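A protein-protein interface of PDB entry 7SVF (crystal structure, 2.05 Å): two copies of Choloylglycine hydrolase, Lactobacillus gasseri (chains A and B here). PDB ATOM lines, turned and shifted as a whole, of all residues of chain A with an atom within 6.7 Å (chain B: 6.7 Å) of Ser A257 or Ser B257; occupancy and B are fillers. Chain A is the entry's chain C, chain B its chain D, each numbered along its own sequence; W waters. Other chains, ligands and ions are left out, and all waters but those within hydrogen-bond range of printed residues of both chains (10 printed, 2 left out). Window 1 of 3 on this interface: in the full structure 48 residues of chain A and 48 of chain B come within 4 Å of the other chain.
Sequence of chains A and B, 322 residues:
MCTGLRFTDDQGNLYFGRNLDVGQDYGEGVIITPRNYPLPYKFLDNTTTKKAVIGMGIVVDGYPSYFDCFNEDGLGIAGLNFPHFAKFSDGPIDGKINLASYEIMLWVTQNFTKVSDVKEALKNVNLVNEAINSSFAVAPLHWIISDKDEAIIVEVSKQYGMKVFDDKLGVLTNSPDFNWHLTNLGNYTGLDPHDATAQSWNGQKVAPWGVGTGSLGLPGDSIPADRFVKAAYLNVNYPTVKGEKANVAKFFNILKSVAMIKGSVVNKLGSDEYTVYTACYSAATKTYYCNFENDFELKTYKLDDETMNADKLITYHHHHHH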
ATOM      1  N   ASN A  19      19.779 -14.560  -2.968  1.00  0.00           N
ATOM      2  CA  ASN A  19      19.089 -15.779  -3.360  1.00  0.00           C
ATOM      3  C   ASN A  19      17.595 -15.531  -3.271  1.00  0.00           C
ATOM      4  O   ASN A  19      17.124 -14.916  -2.315  1.00  0.00           O
ATOM      5  CB  ASN A  19      19.407 -16.944  -2.412  1.00  0.00           C
ATOM      6  CG  ASN A  19      20.816 -17.478  -2.541  1.00  0.00           C
ATOM      7  OD1 ASN A  19      21.483 -17.325  -3.563  1.00  0.00           O
ATOM      8  ND2 ASN A  19      21.271 -18.137  -1.482  1.00  0.00           N
ATOM      9  N   GLY A 220      23.409 -25.841   9.485  1.00  0.00           N
ATOM     10  CA  GLY A 220      23.454 -26.033   8.043  1.00  0.00           C
ATOM     11  C   GLY A 220      22.096 -26.193   7.390  1.00  0.00           C
ATOM     12  O   GLY A 220      22.003 -26.405   6.177  1.00  0.00           O
ATOM     13  N   LYS A 230      24.865 -18.311   9.643  1.00  0.00           N
ATOM     14  CA  LYS A 230      25.927 -18.798   8.772  1.00  0.00           C
ATOM     15  C   LYS A 230      26.321 -17.741   7.739  1.00  0.00           C
ATOM     16  O   LYS A 230      27.510 -17.453   7.558  1.00  0.00           O
ATOM     17  CB  LYS A 230      25.506 -20.110   8.104  1.00  0.00           C
ATOM     18  CG  LYS A 230      26.606 -20.673   7.185  1.00  0.00           C
ATOM     19  CD  LYS A 230      26.430 -22.147   6.896  1.00  0.00           C
ATOM     20  CE  LYS A 230      27.301 -22.571   5.699  1.00  0.00           C
ATOM     21  NZ  LYS A 230      27.358 -24.050   5.590  1.00  0.00           N
ATOM     22  N   LEU A 234      30.041 -16.217   7.510  1.00  0.00           N
ATOM     23  CA  LEU A 234      30.854 -16.380   6.309  1.00  0.00           C
ATOM     24  C   LEU A 234      31.254 -15.030   5.725  1.00  0.00           C
ATOM     25  O   LEU A 234      32.401 -14.848   5.288  1.00  0.00           O
ATOM     26  CB  LEU A 234      30.103 -17.200   5.264  1.00  0.00           C
ATOM     27  CG  LEU A 234      29.750 -18.647   5.591  1.00  0.00           C
ATOM     28  CD1 LEU A 234      28.972 -19.247   4.417  1.00  0.00           C
ATOM     29  CD2 LEU A 234      31.013 -19.462   5.924  1.00  0.00           C
ATOM     30  N   PHE A 252      29.101 -15.475  -5.077  1.00  0.00           N
ATOM     31  CA  PHE A 252      28.377 -16.716  -5.330  1.00  0.00           C
ATOM     32  C   PHE A 252      28.859 -17.854  -4.428  1.00  0.00           C
ATOM     33  O   PHE A 252      28.067 -18.738  -4.085  1.00  0.00           O
ATOM     34  CB  PHE A 252      28.499 -17.103  -6.804  1.00  0.00           C
ATOM     35  CG  PHE A 252      27.541 -16.370  -7.707  1.00  0.00           C
ATOM     36  CD1 PHE A 252      27.820 -15.082  -8.141  1.00  0.00           C
ATOM     37  CD2 PHE A 252      26.364 -16.975  -8.130  1.00  0.00           C
ATOM     38  CE1 PHE A 252      26.931 -14.401  -8.980  1.00  0.00           C
ATOM     39  CE2 PHE A 252      25.474 -16.303  -8.958  1.00  0.00           C
ATOM     40  CZ  PHE A 252      25.760 -15.012  -9.382  1.00  0.00           C
ATOM     41  N   ASN A 253      30.138 -17.862  -4.033  1.00  0.00           N
ATOM     42  CA  ASN A 253      30.587 -18.881  -3.077  1.00  0.00           C
ATOM     43  C   ASN A 253      29.774 -18.800  -1.784  1.00  0.00           C
ATOM     44  O   ASN A 253      29.282 -19.817  -1.269  1.00  0.00           O
ATOM     45  CB  ASN A 253      32.082 -18.722  -2.769  1.00  0.00           C
ATOM     46  CG  ASN A 253      32.983 -19.039  -3.969  1.00  0.00           C
ATOM     47  OD1 ASN A 253      32.591 -19.752  -4.897  1.00  0.00           O
ATOM     48  ND2 ASN A 253      34.197 -18.497  -3.948  1.00  0.00           N
ATOM     49  N   ILE A 254      29.611 -17.582  -1.254  1.00  0.00           N
ATOM     50  CA  ILE A 254      28.897 -17.400   0.008  1.00  0.00           C
ATOM     51  C   ILE A 254      27.427 -17.759  -0.152  1.00  0.00           C
ATOM     52  O   ILE A 254      26.876 -18.538   0.634  1.00  0.00           O
ATOM     53  CB  ILE A 254      29.067 -15.959   0.515  1.00  0.00           C
ATOM     54  CG1 ILE A 254      30.510 -15.724   0.964  1.00  0.00           C
ATOM     55  CG2 ILE A 254      28.099 -15.673   1.671  1.00  0.00           C
ATOM     56  CD1 ILE A 254      30.858 -14.217   1.133  1.00  0.00           C
ATOM     57  N   LEU A 255      26.761 -17.186  -1.167  1.00  0.00           N
ATOM     58  CA  LEU A 255      25.323 -17.400  -1.308  1.00  0.00           C
ATOM     59  C   LEU A 255      24.985 -18.832  -1.724  1.00  0.00           C
ATOM     60  O   LEU A 255      23.923 -19.344  -1.348  1.00  0.00           O
ATOM     61  CB  LEU A 255      24.728 -16.405  -2.304  1.00  0.00           C
ATOM     62  CG  LEU A 255      24.375 -15.023  -1.726  1.00  0.00           C
ATOM     63  CD1 LEU A 255      23.488 -14.261  -2.707  1.00  0.00           C
ATOM     64  CD2 LEU A 255      23.703 -15.134  -0.351  1.00  0.00           C
ATOM     65  N   LYS A 256      25.845 -19.491  -2.507  1.00  0.00           N
ATOM     66  CA  LYS A 256      25.555 -20.884  -2.828  1.00  0.00           C
ATOM     67  C   LYS A 256      25.761 -21.774  -1.609  1.00  0.00           C
ATOM     68  O   LYS A 256      25.141 -22.835  -1.504  1.00  0.00           O
ATOM     69  CB  LYS A 256      26.409 -21.353  -4.006  1.00  0.00           C
ATOM     70  CG  LYS A 256      25.957 -20.729  -5.350  1.00  0.00           C
ATOM     71  CD  LYS A 256      24.447 -20.944  -5.596  1.00  0.00           C
ATOM     72  CE  LYS A 256      24.028 -20.489  -6.999  1.00  0.00           C
ATOM     73  NZ  LYS A 256      22.559 -20.651  -7.249  1.00  0.00           N
ATOM     74  N   SER A 257      26.591 -21.333  -0.668  1.00  0.00           N
ATOM     75  CA  SER A 257      26.805 -22.095   0.552  1.00  0.00           C
ATOM     76  C   SER A 257      25.543 -22.120   1.412  1.00  0.00           C
ATOM     77  O   SER A 257      25.270 -23.123   2.089  1.00  0.00           O
ATOM     78  CB  SER A 257      27.990 -21.503   1.322  1.00  0.00           C
ATOM     79  OG  SER A 257      28.080 -22.045   2.626  1.00  0.00           O
ATOM     80  N   VAL A 258      24.751 -21.041   1.390  1.00  0.00           N
ATOM     81  CA  VAL A 258      23.539 -20.964   2.206  1.00  0.00           C
ATOM     82  C   VAL A 258      22.277 -21.106   1.357  1.00  0.00           C
ATOM     83  O   VAL A 258      21.175 -20.763   1.813  1.00  0.00           O
ATOM     84  CB  VAL A 258      23.491 -19.683   3.058  1.00  0.00           C
ATOM     85  CG1 VAL A 258      24.526 -19.744   4.182  1.00  0.00           C
ATOM     86  CG2 VAL A 258      23.676 -18.439   2.197  1.00  0.00           C
ATOM     87  N   ALA A 259      22.411 -21.604   0.131  1.00  0.00           N
ATOM     88  CA  ALA A 259      21.246 -21.814  -0.716  1.00  0.00           C
ATOM     89  C   ALA A 259      20.328 -22.879  -0.122  1.00  0.00           C
ATOM     90  O   ALA A 259      20.761 -23.772   0.608  1.00  0.00           O
ATOM     91  CB  ALA A 259      21.669 -22.235  -2.121  1.00  0.00           C
ATOM     92  N   ILE A 261      18.385 -26.056  -0.888  1.00  0.00           N
ATOM     93  CA  ILE A 261      18.637 -27.068  -1.910  1.00  0.00           C
ATOM     94  C   ILE A 261      17.354 -27.828  -2.220  1.00  0.00           C
ATOM     95  O   ILE A 261      16.668 -28.307  -1.311  1.00  0.00           O
ATOM     96  CB  ILE A 261      19.749 -28.032  -1.461  1.00  0.00           C
ATOM     97  CG1 ILE A 261      21.027 -27.252  -1.160  1.00  0.00           C
ATOM     98  CG2 ILE A 261      20.016 -29.075  -2.547  1.00  0.00           C
ATOM     99  CD1 ILE A 261      21.428 -26.294  -2.283  1.00  0.00           C
ATOM    100  N   ASN B  19      34.450 -31.562  -5.038  1.00  0.00           N
ATOM    101  CA  ASN B  19      35.148 -30.375  -4.559  1.00  0.00           C
ATOM    102  C   ASN B  19      36.560 -30.772  -4.148  1.00  0.00           C
ATOM    103  O   ASN B  19      36.744 -31.794  -3.486  1.00  0.00           O
ATOM    104  CB  ASN B  19      34.459 -29.764  -3.324  1.00  0.00           C
ATOM    105  CG  ASN B  19      33.110 -29.132  -3.622  1.00  0.00           C
ATOM    106  OD1 ASN B  19      32.853 -28.645  -4.721  1.00  0.00           O
ATOM    107  ND2 ASN B  19      32.231 -29.137  -2.612  1.00  0.00           N
ATOM    108  N   GLY B 220      26.302 -27.525   9.600  1.00  0.00           N
ATOM    109  CA  GLY B 220      26.717 -26.659   8.503  1.00  0.00           C
ATOM    110  C   GLY B 220      28.194 -26.307   8.435  1.00  0.00           C
ATOM    111  O   GLY B 220      28.628 -25.543   7.563  1.00  0.00           O
ATOM    112  N   LYS B 230      25.544 -34.001   5.491  1.00  0.00           N
ATOM    113  CA  LYS B 230      24.773 -33.058   4.683  1.00  0.00           C
ATOM    114  C   LYS B 230      24.783 -33.455   3.207  1.00  0.00           C
ATOM    115  O   LYS B 230      23.732 -33.455   2.553  1.00  0.00           O
ATOM    116  CB  LYS B 230      25.294 -31.632   4.888  1.00  0.00           C
ATOM    117  CG  LYS B 230      24.579 -30.594   4.021  1.00  0.00           C
ATOM    118  CD  LYS B 230      24.543 -29.201   4.638  1.00  0.00           C
ATOM    119  CE  LYS B 230      24.082 -28.193   3.579  1.00  0.00           C
ATOM    120  NZ  LYS B 230      23.994 -26.804   4.111  1.00  0.00           N
ATOM    121  N   LEU B 234      21.453 -34.336   1.190  1.00  0.00           N
ATOM    122  CA  LEU B 234      21.060 -33.578   0.002  1.00  0.00           C
ATOM    123  C   LEU B 234      20.937 -34.482  -1.223  1.00  0.00           C
ATOM    124  O   LEU B 234      19.972 -34.375  -1.990  1.00  0.00           O
ATOM    125  CB  LEU B 234      22.062 -32.451  -0.261  1.00  0.00           C
ATOM    126  CG  LEU B 234      22.092 -31.382   0.843  1.00  0.00           C
ATOM    127  CD1 LEU B 234      23.083 -30.303   0.472  1.00  0.00           C
ATOM    128  CD2 LEU B 234      20.713 -30.790   1.066  1.00  0.00           C
ATOM    129  N   PHE B 252      26.160 -28.949  -9.250  1.00  0.00           N
ATOM    130  CA  PHE B 252      26.846 -27.822  -8.620  1.00  0.00           C
ATOM    131  C   PHE B 252      26.040 -27.251  -7.451  1.00  0.00           C
ATOM    132  O   PHE B 252      26.629 -26.760  -6.482  1.00  0.00           O
ATOM    133  CB  PHE B 252      27.159 -26.735  -9.663  1.00  0.00           C
ATOM    134  CG  PHE B 252      28.415 -27.007 -10.460  1.00  0.00           C
ATOM    135  CD1 PHE B 252      28.394 -27.900 -11.524  1.00  0.00           C
ATOM    136  CD2 PHE B 252      29.618 -26.392 -10.128  1.00  0.00           C
ATOM    137  CE1 PHE B 252      29.560 -28.182 -12.257  1.00  0.00           C
ATOM    138  CE2 PHE B 252      30.788 -26.665 -10.849  1.00  0.00           C
ATOM    139  CZ  PHE B 252      30.755 -27.569 -11.916  1.00  0.00           C
ATOM    140  N   ASN B 253      24.706 -27.317  -7.511  1.00  0.00           N
ATOM    141  CA  ASN B 253      23.894 -26.876  -6.373  1.00  0.00           C
ATOM    142  C   ASN B 253      24.268 -27.644  -5.104  1.00  0.00           C
ATOM    143  O   ASN B 253      24.436 -27.050  -4.031  1.00  0.00           O
ATOM    144  CB  ASN B 253      22.400 -27.051  -6.680  1.00  0.00           C
ATOM    145  CG  ASN B 253      21.893 -26.085  -7.767  1.00  0.00           C
ATOM    146  OD1 ASN B 253      22.485 -25.027  -8.001  1.00  0.00           O
ATOM    147  ND2 ASN B 253      20.796 -26.459  -8.437  1.00  0.00           N
ATOM    148  N   ILE B 254      24.429 -28.964  -5.217  1.00  0.00           N
ATOM    149  CA  ILE B 254      24.720 -29.784  -4.043  1.00  0.00           C
ATOM    150  C   ILE B 254      26.141 -29.529  -3.543  1.00  0.00           C
ATOM    151  O   ILE B 254      26.358 -29.274  -2.354  1.00  0.00           O
ATOM    152  CB  ILE B 254      24.488 -31.273  -4.370  1.00  0.00           C
ATOM    153  CG1 ILE B 254      22.990 -31.556  -4.552  1.00  0.00           C
ATOM    154  CG2 ILE B 254      25.087 -32.178  -3.287  1.00  0.00           C
ATOM    155  CD1 ILE B 254      22.701 -32.873  -5.258  1.00  0.00           C
ATOM    156  N   LEU B 255      27.135 -29.581  -4.443  1.00  0.00           N
ATOM    157  CA  LEU B 255      28.518 -29.461  -3.982  1.00  0.00           C
ATOM    158  C   LEU B 255      28.844 -28.047  -3.503  1.00  0.00           C
ATOM    159  O   LEU B 255      29.637 -27.882  -2.563  1.00  0.00           O
ATOM    160  CB  LEU B 255      29.501 -29.894  -5.075  1.00  0.00           C
ATOM    161  CG  LEU B 255      29.734 -31.413  -5.186  1.00  0.00           C
ATOM    162  CD1 LEU B 255      30.980 -31.684  -5.997  1.00  0.00           C
ATOM    163  CD2 LEU B 255      29.804 -32.105  -3.812  1.00  0.00           C
ATOM    164  N   LYS B 256      28.254 -27.016  -4.122  1.00  0.00           N
ATOM    165  CA  LYS B 256      28.483 -25.669  -3.612  1.00  0.00           C
ATOM    166  C   LYS B 256      27.785 -25.460  -2.272  1.00  0.00           C
ATOM    167  O   LYS B 256      28.229 -24.638  -1.468  1.00  0.00           O
ATOM    168  CB  LYS B 256      28.039 -24.623  -4.635  1.00  0.00           C
ATOM    169  CG  LYS B 256      28.923 -24.587  -5.899  1.00  0.00           C
ATOM    170  CD  LYS B 256      30.422 -24.436  -5.575  1.00  0.00           C
ATOM    171  CE  LYS B 256      31.221 -24.079  -6.839  1.00  0.00           C
ATOM    172  NZ  LYS B 256      32.684 -24.044  -6.581  1.00  0.00           N
ATOM    173  N   SER B 257      26.709 -26.202  -2.012  1.00  0.00           N
ATOM    174  CA  SER B 257      26.086 -26.172  -0.690  1.00  0.00           C
ATOM    175  C   SER B 257      27.064 -26.616   0.399  1.00  0.00           C
ATOM    176  O   SER B 257      27.090 -26.033   1.489  1.00  0.00           O
ATOM    177  CB  SER B 257      24.847 -27.066  -0.680  1.00  0.00           C
ATOM    178  OG  SER B 257      24.261 -27.105   0.606  1.00  0.00           O
ATOM    179  N   VAL B 258      27.866 -27.653   0.134  1.00  0.00           N
ATOM    180  CA  VAL B 258      28.778 -28.197   1.138  1.00  0.00           C
ATOM    181  C   VAL B 258      30.225 -27.757   0.890  1.00  0.00           C
ATOM    182  O   VAL B 258      31.155 -28.332   1.467  1.00  0.00           O
ATOM    183  CB  VAL B 258      28.674 -29.730   1.239  1.00  0.00           C
ATOM    184  CG1 VAL B 258      27.304 -30.141   1.749  1.00  0.00           C
ATOM    185  CG2 VAL B 258      28.985 -30.412  -0.087  1.00  0.00           C
ATOM    186  N   ALA B 259      30.433 -26.739   0.054  1.00  0.00           N
ATOM    187  CA  ALA B 259      31.774 -26.205  -0.151  1.00  0.00           C
ATOM    188  C   ALA B 259      32.364 -25.694   1.160  1.00  0.00           C
ATOM    189  O   ALA B 259      31.654 -25.331   2.100  1.00  0.00           O
ATOM    190  CB  ALA B 259      31.755 -25.073  -1.191  1.00  0.00           C
ATOM    191  N   MET B 260      33.687 -25.681   1.214  1.00  0.00           N
ATOM    192  CA  MET B 260      34.430 -25.114   2.332  1.00  0.00           C
ATOM    193  C   MET B 260      34.760 -23.671   1.953  1.00  0.00           C
ATOM    194  O   MET B 260      35.475 -23.426   0.979  1.00  0.00           O
ATOM    195  CB  MET B 260      35.683 -25.955   2.594  1.00  0.00           C
ATOM    196  CG  MET B 260      36.444 -25.676   3.869  1.00  0.00           C
ATOM    197  SD  MET B 260      37.856 -26.815   4.093  1.00  0.00           S
ATOM    198  CE  MET B 260      37.063 -28.433   4.027  1.00  0.00           C
ATOM    199  N   ILE B 261      34.198 -22.713   2.682  1.00  0.00           N
ATOM    200  CA  ILE B 261      34.196 -21.312   2.257  1.00  0.00           C
ATOM    201  C   ILE B 261      35.440 -20.608   2.788  1.00  0.00           C
ATOM    202  O   ILE B 261      35.745 -20.682   3.983  1.00  0.00           O
ATOM    203  CB  ILE B 261      32.909 -20.609   2.726  1.00  0.00           C
ATOM    204  CG1 ILE B 261      31.687 -21.359   2.184  1.00  0.00           C
ATOM    205  CG2 ILE B 261      32.864 -19.168   2.262  1.00  0.00           C
ATOM    206  CD1 ILE B 261      31.796 -21.682   0.692  1.00  0.00           C
HETATM  207  O   HOH W   1      30.581 -24.236   5.958  1.00  0.00           O
HETATM  208  O   HOH W   2      32.491 -22.404  -3.601  1.00  0.00           O
HETATM  209  O   HOH W   3      21.900 -22.626  -9.072  1.00  0.00           O
HETATM  210  O   HOH W   4      29.072 -24.656   2.697  1.00  0.00           O
HETATM  211  O   HOH W   5      33.840 -21.282  -6.831  1.00  0.00           O
HETATM  212  O   HOH W   6      24.739 -24.072   4.746  1.00  0.00           O
HETATM  213  O   HOH W   7      22.098 -23.291  -5.772  1.00  0.00           O
HETATM  214  O   HOH W   8      23.108 -24.976   1.651  1.00  0.00           O
HETATM  215  O   HOH W   9      24.002 -24.263  -3.807  1.00  0.00           O
HETATM  216  O   HOH W  10      29.957 -22.332  -2.349  1.00  0.00           O
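CB of Ile B261 touches CD2 of Leu A234, 3.9 Å away. CD1 of Ile B261 touches O of Asn A253 (3.7 Å). Lys A256 touches Lys B256 (O to O, 3.6 Å). Ser B257 touches Lys A256. CA of Ser A257 touches O of Lys B256, at 3.5 Å. OG of Ser A257 touches CG1 of Ile B261, 3.7 Å away. Ile A261 touches Leu B234. Ile A261 touches Asn B253 (CD1 to O, 3.6 Å). Ser B257 touches Ile A261.
Of the printed residues of chain B, Lys A230 touches Gly B220. Of the printed residues of chain B, Asn A253 touches Ile B261 (3.7 Å). Ile A254 touches none of the printed residues of chain B. Printed residues of chain B within 4 Å of Ile A261: Leu B234 (3.9 Å), Asn B253 (3.6 Å) and Ser B257 (3.7 Å). Of the printed residues of chain A, Leu B234 touches Ile A261 (3.9 Å). Of chain A, only Lys A256 (3.6 Å), Ser A257 (3.5 Å) and Ile A261 (3.7 Å) come within 4 Å of Ser B257. The nearest residue of chain A that does not touch Ser B257 is Lys A230 (4.6 Å). The nearest printed residue of chain B that does not touch Lys A256 is Asn B253 (4.4 Å).
Hydrophobic or aromatic side chains of chain A that line the printed part of chain B: Leu A234 and Ile A261. Of the 14 printed residues of chain B, 7 touch a printed residue of chain A. Among the printed residues, 13 pairs touch across the chains.
Water W3 bridges the side-chain amide oxygen (OD1) of Asn B253 (2.7 Å) and the side-chain amino group (NZ) of Lys A256 (2.8 Å). Water W5 bridges the side-chain amide oxygen (OD1) of Asn A253 and the side-chain amino group (NZ) of Lys B256. Water W10 bridges the backbone carbonyl oxygen of Asn A253 (2.8 Å) and the backbone carbonyl oxygen of Lys B256 (3.0 Å). Water W1 bridges O of Gly B220 and NZ of Lys A230. Water W7 bridges the side-chain amide oxygen of Asn B253 and the side-chain amino group of Lys A256. Water W2 bridges OD1 of Asn A253 (3.0 Å) and NZ of Lys B256 (3.4 Å).
Leu A234 touches Ile B261, and with the chains exchanged Ile A261 touches Leu B234. Lys A256 touches its own counterpart, Lys B256. Lys A256 touches Ser B257, and with the chains exchanged Ser A257 touches Lys B256. Ser A257 touches its own counterpart, Ser B257. Positions printed for both chains: 19, 220, 230, 234, 252, 253, 254, 255, 256, 257, 258, 259 and 261.
The side-chain amino group (NZ) of Lys A230 sits at hydrogen-bond distance from the backbone carbonyl oxygen (O) of Gly B220 (2.8 Å). O of Gly A220 sits at hydrogen-bond distance from NZ of Lys B230, at 2.9 Å. The backbone carbonyl oxygen (O) of Ser A257 lies close to the backbone carbonyl oxygen (O) of Ser B257. The backbone NH (N) of Gly A220 lies close to the backbone NH (N) of Gly B220, at 3.3 Å.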
